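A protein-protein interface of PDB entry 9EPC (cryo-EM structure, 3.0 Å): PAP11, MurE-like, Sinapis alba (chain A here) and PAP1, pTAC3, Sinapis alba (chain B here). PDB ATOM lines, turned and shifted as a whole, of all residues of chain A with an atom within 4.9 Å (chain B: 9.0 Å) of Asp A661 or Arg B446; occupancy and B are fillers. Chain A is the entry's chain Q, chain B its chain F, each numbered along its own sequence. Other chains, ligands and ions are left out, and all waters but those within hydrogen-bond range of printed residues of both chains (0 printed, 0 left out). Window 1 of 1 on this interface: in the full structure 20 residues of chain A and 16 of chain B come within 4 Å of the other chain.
Leu B433 touches Pro A630 (CD2 to CG, 3.7 Å). Pro A630 touches Tyr B436. OD1 of Asp A657 touches CG2 of Val B450, at 3.6 Å. C of Arg B448 touches OD2 of Asp A660 (3.2 Å). Ser A664 touches Tyr B432 (O to CB, 3.2 Å). OG of Ser A664 touches CB of Tyr B436 (3.9 Å). Gly A665 touches Tyr B432.
Hydrophobic or aromatic side chains of chain A within 4 Å of the printed part of chain B: Pro A630. Of the 22 printed residues of chain B, 7 touch a printed residue of chain A. Hydrophobic or aromatic side chains of chain B within 4 Å of the printed part of chain A: Tyr B432, Leu B433, Tyr B436, Trp B449 and Val B450. Along chain B the printed residues that touch a printed residue of chain A span positions 432 to 450. Among the printed residues, 15 pairs touch across the chains. Among the printed residues, Asp or Glu carboxylates within 4 Å of a Lys or Arg side-chain nitrogen of the other chain: Glu A653 with Arg B448 (3.1 Å), Asp A661 with Arg B446 (3.6 Å) and Asp A661 with Arg B448 (2.8 Å).
The side-chain carboxylate (OE1) of Glu A653 lies within salt-bridge range of the guanidinium group (NH2) of Arg A629 (2.8 Å). The guanidinium group of Arg A629 lies within salt-bridge range of the side-chain carboxylate of Asp A661, 3.0 Å away. The side-chain hydroxyl (OH) of Tyr B436 is in hydrogen-bond range of the backbone carbonyl oxygen (O) of Gly B441, at 2.6 Å. NH1 of Arg B446 is in salt-bridge range of OE1 of Glu B439.
OE2 of Glu A653 is in salt-bridge range of NH2 of Arg B448. The backbone carbonyl oxygen (O) of Asp A657 sits at hydrogen-bond distance from the guanidinium group (NH1) of Arg B448, 2.8 Å away. The side-chain carboxylate (OD2) of Asp A660 lies within hydrogen-bond range of the backbone NH (N) of Trp B449. OD2 of Asp A660 sits at hydrogen-bond distance from N of Val B450 (3.3 Å). OD2 of Asp A661 sits at hydrogen-bond distance from OH of Tyr B436, 3.2 Å away. The guanidinium group (NE) of Arg B446 lies within salt-bridge range of the side-chain carboxylate (OD1) of Asp A661 (3.6 Å). NH1 of Arg B448 lies within salt-bridge range of OD1 of Asp A661 (2.8 Å). The guanidinium group (NH1) of Arg B446 lies close to the side-chain hydroxyl (OG) of Ser A664, 3.5 Å away.
Of chain B, only Tyr B436 (3.2 Å), Arg B446 (3.3 Å) and Arg B448 (2.8 Å) come within 4 Å of Asp A661. Of chain A, only Asp A661 (3.3 Å) and Ser A664 (3.4 Å) come within 4 Å of Arg B446. Printed residues of chain B within 4 Å of Asp A660: Arg B448 (3.2 Å), Trp B449 (2.5 Å) and Val B450 (3.3 Å). Of the printed residues of chain A, Val B450 touches Asp A657 (3.6 Å) and Asp A660 (3.3 Å). Printed residues of chain B within 4 Å of Pro A630: Leu B433 (3.7 Å) and Tyr B436 (3.4 Å). Of the printed residues of chain B, Glu A653 touches Arg B448 (3.1 Å). The nearest residue of chain B that does not touch Asp A661 is Gly B441 (4.8 Å).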
ATOM      1  N   ARG A 629       8.931 -17.793  23.295  1.00  0.00           N
ATOM      2  CA  ARG A 629       8.610 -17.354  21.938  1.00  0.00           C
ATOM      3  C   ARG A 629       7.155 -16.936  21.772  1.00  0.00           C
ATOM      4  O   ARG A 629       6.913 -15.854  21.209  1.00  0.00           O
ATOM      5  CB  ARG A 629       9.009 -18.450  20.945  1.00  0.00           C
ATOM      6  CG  ARG A 629      10.503 -18.723  20.925  1.00  0.00           C
ATOM      7  CD  ARG A 629      10.827 -19.978  20.145  1.00  0.00           C
ATOM      8  NE  ARG A 629      12.262 -20.221  20.075  1.00  0.00           N
ATOM      9  CZ  ARG A 629      12.806 -21.315  19.561  1.00  0.00           C
ATOM     10  NH1 ARG A 629      12.061 -22.295  19.079  1.00  0.00           N
ATOM     11  NH2 ARG A 629      14.131 -21.429  19.534  1.00  0.00           N
ATOM     12  N   PRO A 630       6.151 -17.705  22.210  1.00  0.00           N
ATOM     13  CA  PRO A 630       4.773 -17.206  22.099  1.00  0.00           C
ATOM     14  C   PRO A 630       4.523 -15.944  22.901  1.00  0.00           C
ATOM     15  O   PRO A 630       3.687 -15.123  22.506  1.00  0.00           O
ATOM     16  CB  PRO A 630       3.933 -18.380  22.617  1.00  0.00           C
ATOM     17  CG  PRO A 630       4.850 -19.125  23.496  1.00  0.00           C
ATOM     18  CD  PRO A 630       6.183 -19.040  22.829  1.00  0.00           C
ATOM     19  N   GLU A 653      18.718 -24.510  14.582  1.00  0.00           N
ATOM     20  CA  GLU A 653      17.282 -24.679  14.433  1.00  0.00           C
ATOM     21  C   GLU A 653      16.791 -23.975  13.174  1.00  0.00           C
ATOM     22  O   GLU A 653      17.372 -22.984  12.724  1.00  0.00           O
ATOM     23  CB  GLU A 653      16.549 -24.138  15.662  1.00  0.00           C
ATOM     24  CG  GLU A 653      15.092 -24.556  15.758  1.00  0.00           C
ATOM     25  CD  GLU A 653      14.428 -24.072  17.031  1.00  0.00           C
ATOM     26  OE1 GLU A 653      15.105 -23.400  17.836  1.00  0.00           O
ATOM     27  OE2 GLU A 653      13.231 -24.364  17.228  1.00  0.00           O
ATOM     28  N   ASP A 657      10.790 -22.616  11.824  1.00  0.00           N
ATOM     29  CA  ASP A 657      10.248 -23.269  13.010  1.00  0.00           C
ATOM     30  C   ASP A 657      10.156 -22.299  14.178  1.00  0.00           C
ATOM     31  O   ASP A 657       9.174 -22.307  14.928  1.00  0.00           O
ATOM     32  CB  ASP A 657      11.107 -24.475  13.382  1.00  0.00           C
ATOM     33  CG  ASP A 657      11.045 -25.575  12.345  1.00  0.00           C
ATOM     34  OD1 ASP A 657      10.326 -25.403  11.339  1.00  0.00           O
ATOM     35  OD2 ASP A 657      11.714 -26.612  12.537  1.00  0.00           O
ATOM     36  N   ILE A 658      11.174 -21.453  14.348  1.00  0.00           N
ATOM     37  CA  ILE A 658      11.148 -20.464  15.421  1.00  0.00           C
ATOM     38  C   ILE A 658       9.983 -19.507  15.226  1.00  0.00           C
ATOM     39  O   ILE A 658       9.270 -19.169  16.180  1.00  0.00           O
ATOM     40  CB  ILE A 658      12.490 -19.716  15.486  1.00  0.00           C
ATOM     41  CG1 ILE A 658      13.646 -20.709  15.597  1.00  0.00           C
ATOM     42  CG2 ILE A 658      12.503 -18.753  16.657  1.00  0.00           C
ATOM     43  CD1 ILE A 658      15.005 -20.056  15.591  1.00  0.00           C
ATOM     44  N   LEU A 659       9.766 -19.059  13.989  1.00  0.00           N
ATOM     45  CA  LEU A 659       8.633 -18.185  13.710  1.00  0.00           C
ATOM     46  C   LEU A 659       7.309 -18.896  13.943  1.00  0.00           C
ATOM     47  O   LEU A 659       6.324 -18.260  14.337  1.00  0.00           O
ATOM     48  CB  LEU A 659       8.713 -17.665  12.277  1.00  0.00           C
ATOM     49  CG  LEU A 659       9.932 -16.805  11.952  1.00  0.00           C
ATOM     50  CD1 LEU A 659       9.933 -16.416  10.487  1.00  0.00           C
ATOM     51  CD2 LEU A 659       9.959 -15.569  12.831  1.00  0.00           C
ATOM     52  N   ASP A 660       7.259 -20.208  13.700  1.00  0.00           N
ATOM     53  CA  ASP A 660       6.032 -20.952  13.959  1.00  0.00           C
ATOM     54  C   ASP A 660       5.698 -20.955  15.443  1.00  0.00           C
ATOM     55  O   ASP A 660       4.528 -20.843  15.825  1.00  0.00           O
ATOM     56  CB  ASP A 660       6.154 -22.378  13.434  1.00  0.00           C
ATOM     57  CG  ASP A 660       4.813 -23.065  13.314  1.00  0.00           C
ATOM     58  OD1 ASP A 660       3.785 -22.413  13.591  1.00  0.00           O
ATOM     59  OD2 ASP A 660       4.781 -24.254  12.938  1.00  0.00           O
ATOM     60  N   ASP A 661       6.714 -21.086  16.298  1.00  0.00           N
ATOM     61  CA  ASP A 661       6.481 -20.974  17.732  1.00  0.00           C
ATOM     62  C   ASP A 661       5.983 -19.584  18.094  1.00  0.00           C
ATOM     63  O   ASP A 661       5.145 -19.431  18.990  1.00  0.00           O
ATOM     64  CB  ASP A 661       7.758 -21.303  18.500  1.00  0.00           C
ATOM     65  CG  ASP A 661       8.142 -22.758  18.381  1.00  0.00           C
ATOM     66  OD1 ASP A 661       7.418 -23.503  17.691  1.00  0.00           O
ATOM     67  OD2 ASP A 661       9.162 -23.159  18.978  1.00  0.00           O
ATOM     68  N   MET A 662       6.490 -18.557  17.412  1.00  0.00           N
ATOM     69  CA  MET A 662       6.006 -17.202  17.651  1.00  0.00           C
ATOM     70  C   MET A 662       4.528 -17.078  17.308  1.00  0.00           C
ATOM     71  O   MET A 662       3.742 -16.531  18.089  1.00  0.00           O
ATOM     72  CB  MET A 662       6.832 -16.201  16.846  1.00  0.00           C
ATOM     73  CG  MET A 662       8.189 -15.904  17.451  1.00  0.00           C
ATOM     74  SD  MET A 662       9.034 -14.559  16.602  1.00  0.00           S
ATOM     75  CE  MET A 662      10.569 -14.524  17.499  1.00  0.00           C
ATOM     76  N   LEU A 663       4.126 -17.601  16.149  1.00  0.00           N
ATOM     77  CA  LEU A 663       2.735 -17.488  15.730  1.00  0.00           C
ATOM     78  C   LEU A 663       1.793 -18.243  16.651  1.00  0.00           C
ATOM     79  O   LEU A 663       0.595 -17.943  16.675  1.00  0.00           O
ATOM     80  CB  LEU A 663       2.577 -17.993  14.300  1.00  0.00           C
ATOM     81  CG  LEU A 663       3.378 -17.212  13.263  1.00  0.00           C
ATOM     82  CD1 LEU A 663       3.181 -17.809  11.887  1.00  0.00           C
ATOM     83  CD2 LEU A 663       2.968 -15.752  13.279  1.00  0.00           C
ATOM     84  N   SER A 664       2.302 -19.217  17.407  1.00  0.00           N
ATOM     85  CA  SER A 664       1.458 -19.914  18.367  1.00  0.00           C
ATOM     86  C   SER A 664       0.927 -18.979  19.444  1.00  0.00           C
ATOM     87  O   SER A 664      -0.118 -19.262  20.036  1.00  0.00           O
ATOM     88  CB  SER A 664       2.226 -21.066  19.012  1.00  0.00           C
ATOM     89  OG  SER A 664       1.414 -21.744  19.953  1.00  0.00           O
ATOM     90  N   GLY A 665       1.625 -17.874  19.709  1.00  0.00           N
ATOM     91  CA  GLY A 665       1.137 -16.919  20.687  1.00  0.00           C
ATOM     92  C   GLY A 665      -0.166 -16.265  20.279  1.00  0.00           C
ATOM     93  O   GLY A 665      -1.000 -15.950  21.131  1.00  0.00           O
ATOM     94  N   ARG B 407      -5.977 -28.748  14.596  1.00  0.00           N
ATOM     95  CA  ARG B 407      -5.721 -27.351  14.896  1.00  0.00           C
ATOM     96  C   ARG B 407      -7.029 -26.660  15.273  1.00  0.00           C
ATOM     97  O   ARG B 407      -8.124 -27.144  14.975  1.00  0.00           O
ATOM     98  CB  ARG B 407      -5.069 -26.658  13.700  1.00  0.00           C
ATOM     99  CG  ARG B 407      -4.437 -25.316  14.022  1.00  0.00           C
ATOM    100  CD  ARG B 407      -4.308 -24.456  12.780  1.00  0.00           C
ATOM    101  NE  ARG B 407      -4.011 -23.070  13.117  1.00  0.00           N
ATOM    102  CZ  ARG B 407      -3.981 -22.075  12.242  1.00  0.00           C
ATOM    103  NH1 ARG B 407      -4.228 -22.276  10.958  1.00  0.00           N
ATOM    104  NH2 ARG B 407      -3.699 -20.847  12.666  1.00  0.00           N
ATOM    105  N   TYR B 409      -8.224 -26.653  18.054  1.00  0.00           N
ATOM    106  CA  TYR B 409      -8.726 -27.387  19.215  1.00  0.00           C
ATOM    107  C   TYR B 409     -10.230 -27.648  19.112  1.00  0.00           C
ATOM    108  O   TYR B 409     -11.029 -27.203  19.937  1.00  0.00           O
ATOM    109  CB  TYR B 409      -8.370 -26.659  20.512  1.00  0.00           C
ATOM    110  CG  TYR B 409      -6.939 -26.880  20.926  1.00  0.00           C
ATOM    111  CD1 TYR B 409      -5.912 -26.135  20.368  1.00  0.00           C
ATOM    112  CD2 TYR B 409      -6.612 -27.848  21.863  1.00  0.00           C
ATOM    113  CE1 TYR B 409      -4.600 -26.341  20.738  1.00  0.00           C
ATOM    114  CE2 TYR B 409      -5.305 -28.060  22.242  1.00  0.00           C
ATOM    115  CZ  TYR B 409      -4.303 -27.304  21.677  1.00  0.00           C
ATOM    116  OH  TYR B 409      -2.999 -27.512  22.053  1.00  0.00           O
ATOM    117  N   TYR B 432      -3.296 -19.111  24.523  1.00  0.00           N
ATOM    118  CA  TYR B 432      -2.313 -19.673  23.602  1.00  0.00           C
ATOM    119  C   TYR B 432      -0.976 -19.995  24.256  1.00  0.00           C
ATOM    120  O   TYR B 432      -0.291 -20.935  23.838  1.00  0.00           O
ATOM    121  CB  TYR B 432      -2.082 -18.710  22.437  1.00  0.00           C
ATOM    122  CG  TYR B 432      -3.339 -18.323  21.700  1.00  0.00           C
ATOM    123  CD1 TYR B 432      -3.967 -19.216  20.846  1.00  0.00           C
ATOM    124  CD2 TYR B 432      -3.890 -17.060  21.849  1.00  0.00           C
ATOM    125  CE1 TYR B 432      -5.114 -18.865  20.168  1.00  0.00           C
ATOM    126  CE2 TYR B 432      -5.034 -16.699  21.172  1.00  0.00           C
ATOM    127  CZ  TYR B 432      -5.642 -17.604  20.333  1.00  0.00           C
ATOM    128  OH  TYR B 432      -6.786 -17.250  19.656  1.00  0.00           O
ATOM    129  N   LEU B 433      -0.588 -19.227  25.277  1.00  0.00           N
ATOM    130  CA  LEU B 433       0.640 -19.542  25.999  1.00  0.00           C
ATOM    131  C   LEU B 433       0.543 -20.907  26.669  1.00  0.00           C
ATOM    132  O   LEU B 433       1.496 -21.693  26.634  1.00  0.00           O
ATOM    133  CB  LEU B 433       0.939 -18.451  27.028  1.00  0.00           C
ATOM    134  CG  LEU B 433       2.280 -18.488  27.770  1.00  0.00           C
ATOM    135  CD1 LEU B 433       2.193 -19.289  29.065  1.00  0.00           C
ATOM    136  CD2 LEU B 433       3.383 -19.037  26.877  1.00  0.00           C
ATOM    137  N   ALA B 434      -0.604 -21.207  27.284  1.00  0.00           N
ATOM    138  CA  ALA B 434      -0.795 -22.524  27.880  1.00  0.00           C
ATOM    139  C   ALA B 434      -0.793 -23.613  26.816  1.00  0.00           C
ATOM    140  O   ALA B 434      -0.250 -24.703  27.033  1.00  0.00           O
ATOM    141  CB  ALA B 434      -2.098 -22.557  28.678  1.00  0.00           C
ATOM    142  N   ARG B 435      -1.400 -23.336  25.660  1.00  0.00           N
ATOM    143  CA  ARG B 435      -1.396 -24.307  24.571  1.00  0.00           C
ATOM    144  C   ARG B 435       0.019 -24.587  24.090  1.00  0.00           C
ATOM    145  O   ARG B 435       0.369 -25.735  23.794  1.00  0.00           O
ATOM    146  CB  ARG B 435      -2.263 -23.807  23.418  1.00  0.00           C
ATOM    147  CG  ARG B 435      -3.747 -23.777  23.723  1.00  0.00           C
ATOM    148  CD  ARG B 435      -4.534 -23.324  22.510  1.00  0.00           C
ATOM    149  NE  ARG B 435      -5.972 -23.420  22.722  1.00  0.00           N
ATOM    150  CZ  ARG B 435      -6.882 -23.110  21.809  1.00  0.00           C
ATOM    151  NH1 ARG B 435      -6.537 -22.681  20.606  1.00  0.00           N
ATOM    152  NH2 ARG B 435      -8.171 -23.233  22.110  1.00  0.00           N
ATOM    153  N   TYR B 436       0.848 -23.548  23.998  1.00  0.00           N
ATOM    154  CA  TYR B 436       2.243 -23.752  23.626  1.00  0.00           C
ATOM    155  C   TYR B 436       2.964 -24.607  24.658  1.00  0.00           C
ATOM    156  O   TYR B 436       3.774 -25.472  24.305  1.00  0.00           O
ATOM    157  CB  TYR B 436       2.940 -22.405  23.461  1.00  0.00           C
ATOM    158  CG  TYR B 436       4.396 -22.508  23.083  1.00  0.00           C
ATOM    159  CD1 TYR B 436       4.780 -22.619  21.758  1.00  0.00           C
ATOM    160  CD2 TYR B 436       5.387 -22.487  24.051  1.00  0.00           C
ATOM    161  CE1 TYR B 436       6.107 -22.710  21.408  1.00  0.00           C
ATOM    162  CE2 TYR B 436       6.716 -22.577  23.711  1.00  0.00           C
ATOM    163  CZ  TYR B 436       7.071 -22.689  22.388  1.00  0.00           C
ATOM    164  OH  TYR B 436       8.399 -22.780  22.045  1.00  0.00           O
ATOM    165  N   VAL B 437       2.688 -24.373  25.942  1.00  0.00           N
ATOM    166  CA  VAL B 437       3.342 -25.133  27.001  1.00  0.00           C
ATOM    167  C   VAL B 437       2.936 -26.599  26.941  1.00  0.00           C
ATOM    168  O   VAL B 437       3.781 -27.498  27.024  1.00  0.00           O
ATOM    169  CB  VAL B 437       3.022 -24.514  28.373  1.00  0.00           C
ATOM    170  CG1 VAL B 437       3.406 -25.465  29.491  1.00  0.00           C
ATOM    171  CG2 VAL B 437       3.739 -23.187  28.530  1.00  0.00           C
ATOM    172  N   GLU B 438       1.637 -26.865  26.784  1.00  0.00           N
ATOM    173  CA  GLU B 438       1.155 -28.240  26.831  1.00  0.00           C
ATOM    174  C   GLU B 438       1.603 -29.060  25.630  1.00  0.00           C
ATOM    175  O   GLU B 438       1.662 -30.291  25.726  1.00  0.00           O
ATOM    176  CB  GLU B 438      -0.370 -28.264  26.935  1.00  0.00           C
ATOM    177  CG  GLU B 438      -1.084 -27.831  25.673  1.00  0.00           C
ATOM    178  CD  GLU B 438      -2.589 -27.872  25.816  1.00  0.00           C
ATOM    179  OE1 GLU B 438      -3.074 -28.070  26.949  1.00  0.00           O
ATOM    180  OE2 GLU B 438      -3.288 -27.708  24.795  1.00  0.00           O
ATOM    181  N   GLU B 439       1.913 -28.422  24.506  1.00  0.00           N
ATOM    182  CA  GLU B 439       2.370 -29.148  23.322  1.00  0.00           C
ATOM    183  C   GLU B 439       3.890 -29.254  23.286  1.00  0.00           C
ATOM    184  O   GLU B 439       4.520 -29.043  22.251  1.00  0.00           O
ATOM    185  CB  GLU B 439       1.841 -28.470  22.066  1.00  0.00           C
ATOM    186  CG  GLU B 439       0.329 -28.394  21.986  1.00  0.00           C
ATOM    187  CD  GLU B 439      -0.146 -27.500  20.859  1.00  0.00           C
ATOM    188  OE1 GLU B 439       0.693 -26.787  20.268  1.00  0.00           O
ATOM    189  OE2 GLU B 439      -1.358 -27.507  20.561  1.00  0.00           O
ATOM    190  N   GLY B 440       4.483 -29.610  24.425  1.00  0.00           N
ATOM    191  CA  GLY B 440       5.920 -29.765  24.558  1.00  0.00           C
ATOM    192  C   GLY B 440       6.751 -28.634  23.987  1.00  0.00           C
ATOM    193  O   GLY B 440       7.910 -28.837  23.611  1.00  0.00           O
ATOM    194  N   GLY B 441       6.178 -27.430  23.929  1.00  0.00           N
ATOM    195  CA  GLY B 441       6.836 -26.333  23.244  1.00  0.00           C
ATOM    196  C   GLY B 441       8.025 -25.756  23.979  1.00  0.00           C
ATOM    197  O   GLY B 441       8.816 -25.025  23.374  1.00  0.00           O
ATOM    198  N   LEU B 442       8.177 -26.069  25.264  1.00  0.00           N
ATOM    199  CA  LEU B 442       9.249 -25.473  26.050  1.00  0.00           C
ATOM    200  C   LEU B 442      10.608 -26.022  25.643  1.00  0.00           C
ATOM    201  O   LEU B 442      11.487 -25.263  25.225  1.00  0.00           O
ATOM    202  CB  LEU B 442       9.022 -25.705  27.545  1.00  0.00           C
ATOM    203  CG  LEU B 442       7.721 -25.157  28.128  1.00  0.00           C
ATOM    204  CD1 LEU B 442       6.652 -26.231  28.126  1.00  0.00           C
ATOM    205  CD2 LEU B 442       7.949 -24.619  29.529  1.00  0.00           C
ATOM    206  N   THR B 443      10.800 -27.334  25.769  1.00  0.00           N
ATOM    207  CA  THR B 443      12.102 -27.910  25.459  1.00  0.00           C
ATOM    208  C   THR B 443      11.994 -29.211  24.674  1.00  0.00           C
ATOM    209  O   THR B 443      12.890 -29.537  23.889  1.00  0.00           O
ATOM    210  CB  THR B 443      12.898 -28.142  26.746  1.00  0.00           C
ATOM    211  OG1 THR B 443      14.139 -28.789  26.435  1.00  0.00           O
ATOM    212  CG2 THR B 443      12.109 -29.008  27.719  1.00  0.00           C
ATOM    213  N   GLY B 444      10.912 -29.961  24.869  1.00  0.00           N
ATOM    214  CA  GLY B 444      10.832 -31.275  24.264  1.00  0.00           C
ATOM    215  C   GLY B 444      10.669 -31.256  22.758  1.00  0.00           C
ATOM    216  O   GLY B 444      11.603 -31.598  22.026  1.00  0.00           O
ATOM    217  N   GLU B 445       9.496 -30.828  22.291  1.00  0.00           N
ATOM    218  CA  GLU B 445       9.180 -30.769  20.867  1.00  0.00           C
ATOM    219  C   GLU B 445       7.780 -30.210  20.666  1.00  0.00           C
ATOM    220  O   GLU B 445       6.912 -30.367  21.531  1.00  0.00           O
ATOM    221  CB  GLU B 445       9.288 -32.154  20.221  1.00  0.00           C
ATOM    222  CG  GLU B 445       8.373 -33.210  20.826  1.00  0.00           C
ATOM    223  CD  GLU B 445       6.991 -33.223  20.201  1.00  0.00           C
ATOM    224  OE1 GLU B 445       6.818 -32.619  19.121  1.00  0.00           O
ATOM    225  OE2 GLU B 445       6.076 -33.834  20.790  1.00  0.00           O
ATOM    226  N   ARG B 446       7.540 -29.581  19.523  1.00  0.00           N
ATOM    227  CA  ARG B 446       6.225 -29.068  19.177  1.00  0.00           C
ATOM    228  C   ARG B 446       5.893 -29.473  17.751  1.00  0.00           C
ATOM    229  O   ARG B 446       6.749 -29.401  16.864  1.00  0.00           O
ATOM    230  CB  ARG B 446       6.169 -27.542  19.323  1.00  0.00           C
ATOM    231  CG  ARG B 446       4.969 -26.897  18.654  1.00  0.00           C
ATOM    232  CD  ARG B 446       5.003 -25.388  18.796  1.00  0.00           C
ATOM    233  NE  ARG B 446       4.058 -24.740  17.895  1.00  0.00           N
ATOM    234  CZ  ARG B 446       2.761 -24.608  18.140  1.00  0.00           C
ATOM    235  NH1 ARG B 446       2.217 -25.078  19.250  1.00  0.00           N
ATOM    236  NH2 ARG B 446       1.992 -23.993  17.248  1.00  0.00           N
ATOM    237  N   LYS B 447       4.656 -29.907  17.533  1.00  0.00           N
ATOM    238  CA  LYS B 447       4.202 -30.215  16.181  1.00  0.00           C
ATOM    239  C   LYS B 447       4.055 -28.898  15.434  1.00  0.00           C
ATOM    240  O   LYS B 447       3.053 -28.195  15.574  1.00  0.00           O
ATOM    241  CB  LYS B 447       2.891 -30.992  16.213  1.00  0.00           C
ATOM    242  CG  LYS B 447       2.583 -31.756  14.930  1.00  0.00           C
ATOM    243  CD  LYS B 447       1.954 -30.869  13.867  1.00  0.00           C
ATOM    244  CE  LYS B 447       1.929 -31.563  12.518  1.00  0.00           C
ATOM    245  NZ  LYS B 447       3.298 -31.862  12.020  1.00  0.00           N
ATOM    246  N   ARG B 448       5.060 -28.560  14.636  1.00  0.00           N
ATOM    247  CA  ARG B 448       5.106 -27.277  13.955  1.00  0.00           C
ATOM    248  C   ARG B 448       4.408 -27.366  12.606  1.00  0.00           C
ATOM    249  O   ARG B 448       4.608 -28.321  11.851  1.00  0.00           O
ATOM    250  CB  ARG B 448       6.555 -26.830  13.776  1.00  0.00           C
ATOM    251  CG  ARG B 448       7.326 -26.783  15.078  1.00  0.00           C
ATOM    252  CD  ARG B 448       8.820 -26.821  14.836  1.00  0.00           C
ATOM    253  NE  ARG B 448       9.569 -26.890  16.084  1.00  0.00           N
ATOM    254  CZ  ARG B 448       9.954 -25.833  16.783  1.00  0.00           C
ATOM    255  NH1 ARG B 448       9.673 -24.603  16.386  1.00  0.00           N
ATOM    256  NH2 ARG B 448      10.639 -26.013  17.908  1.00  0.00           N
ATOM    257  N   TRP B 449       3.586 -26.359  12.308  1.00  0.00           N
ATOM    258  CA  TRP B 449       2.801 -26.328  11.082  1.00  0.00           C
ATOM    259  C   TRP B 449       3.528 -25.648   9.932  1.00  0.00           C
ATOM    260  O   TRP B 449       2.878 -25.107   9.029  1.00  0.00           O
ATOM    261  CB  TRP B 449       1.456 -25.651  11.335  1.00  0.00           C
ATOM    262  CG  TRP B 449       0.342 -26.621  11.523  1.00  0.00           C
ATOM    263  CD1 TRP B 449      -0.533 -27.056  10.573  1.00  0.00           C
ATOM    264  CD2 TRP B 449      -0.014 -27.290  12.734  1.00  0.00           C
ATOM    265  NE1 TRP B 449      -1.418 -27.953  11.120  1.00  0.00           N
ATOM    266  CE2 TRP B 449      -1.120 -28.114  12.446  1.00  0.00           C
ATOM    267  CE3 TRP B 449       0.492 -27.270  14.036  1.00  0.00           C
ATOM    268  CZ2 TRP B 449      -1.727 -28.910  13.411  1.00  0.00           C
ATOM    269  CZ3 TRP B 449      -0.111 -28.062  14.992  1.00  0.00           C
ATOM    270  CH2 TRP B 449      -1.209 -28.870  14.675  1.00  0.00           C
ATOM    271  N   VAL B 450       4.856 -25.653   9.939  1.00  0.00           N
ATOM    272  CA  VAL B 450       5.623 -25.100   8.828  1.00  0.00           C
ATOM    273  C   VAL B 450       5.496 -26.042   7.638  1.00  0.00           C
ATOM    274  O   VAL B 450       5.877 -27.217   7.738  1.00  0.00           O
ATOM    275  CB  VAL B 450       7.096 -24.896   9.208  1.00  0.00           C
ATOM    276  CG1 VAL B 450       7.898 -24.484   7.987  1.00  0.00           C
ATOM    277  CG2 VAL B 450       7.219 -23.857  10.302  1.00  0.00           C
ATOM    278  N   LEU B 458       1.727 -32.658   5.966  1.00  0.00           N
ATOM    279  CA  LEU B 458       1.929 -31.857   7.168  1.00  0.00           C
ATOM    280  C   LEU B 458       0.839 -32.123   8.198  1.00  0.00           C
ATOM    281  O   LEU B 458       1.113 -32.217   9.400  1.00  0.00           O
ATOM    282  CB  LEU B 458       1.972 -30.374   6.805  1.00  0.00           C
ATOM    283  CG  LEU B 458       2.091 -29.414   7.988  1.00  0.00           C
ATOM    284  CD1 LEU B 458       3.361 -29.693   8.773  1.00  0.00           C
ATOM    285  CD2 LEU B 458       2.056 -27.973   7.513  1.00  0.00           C
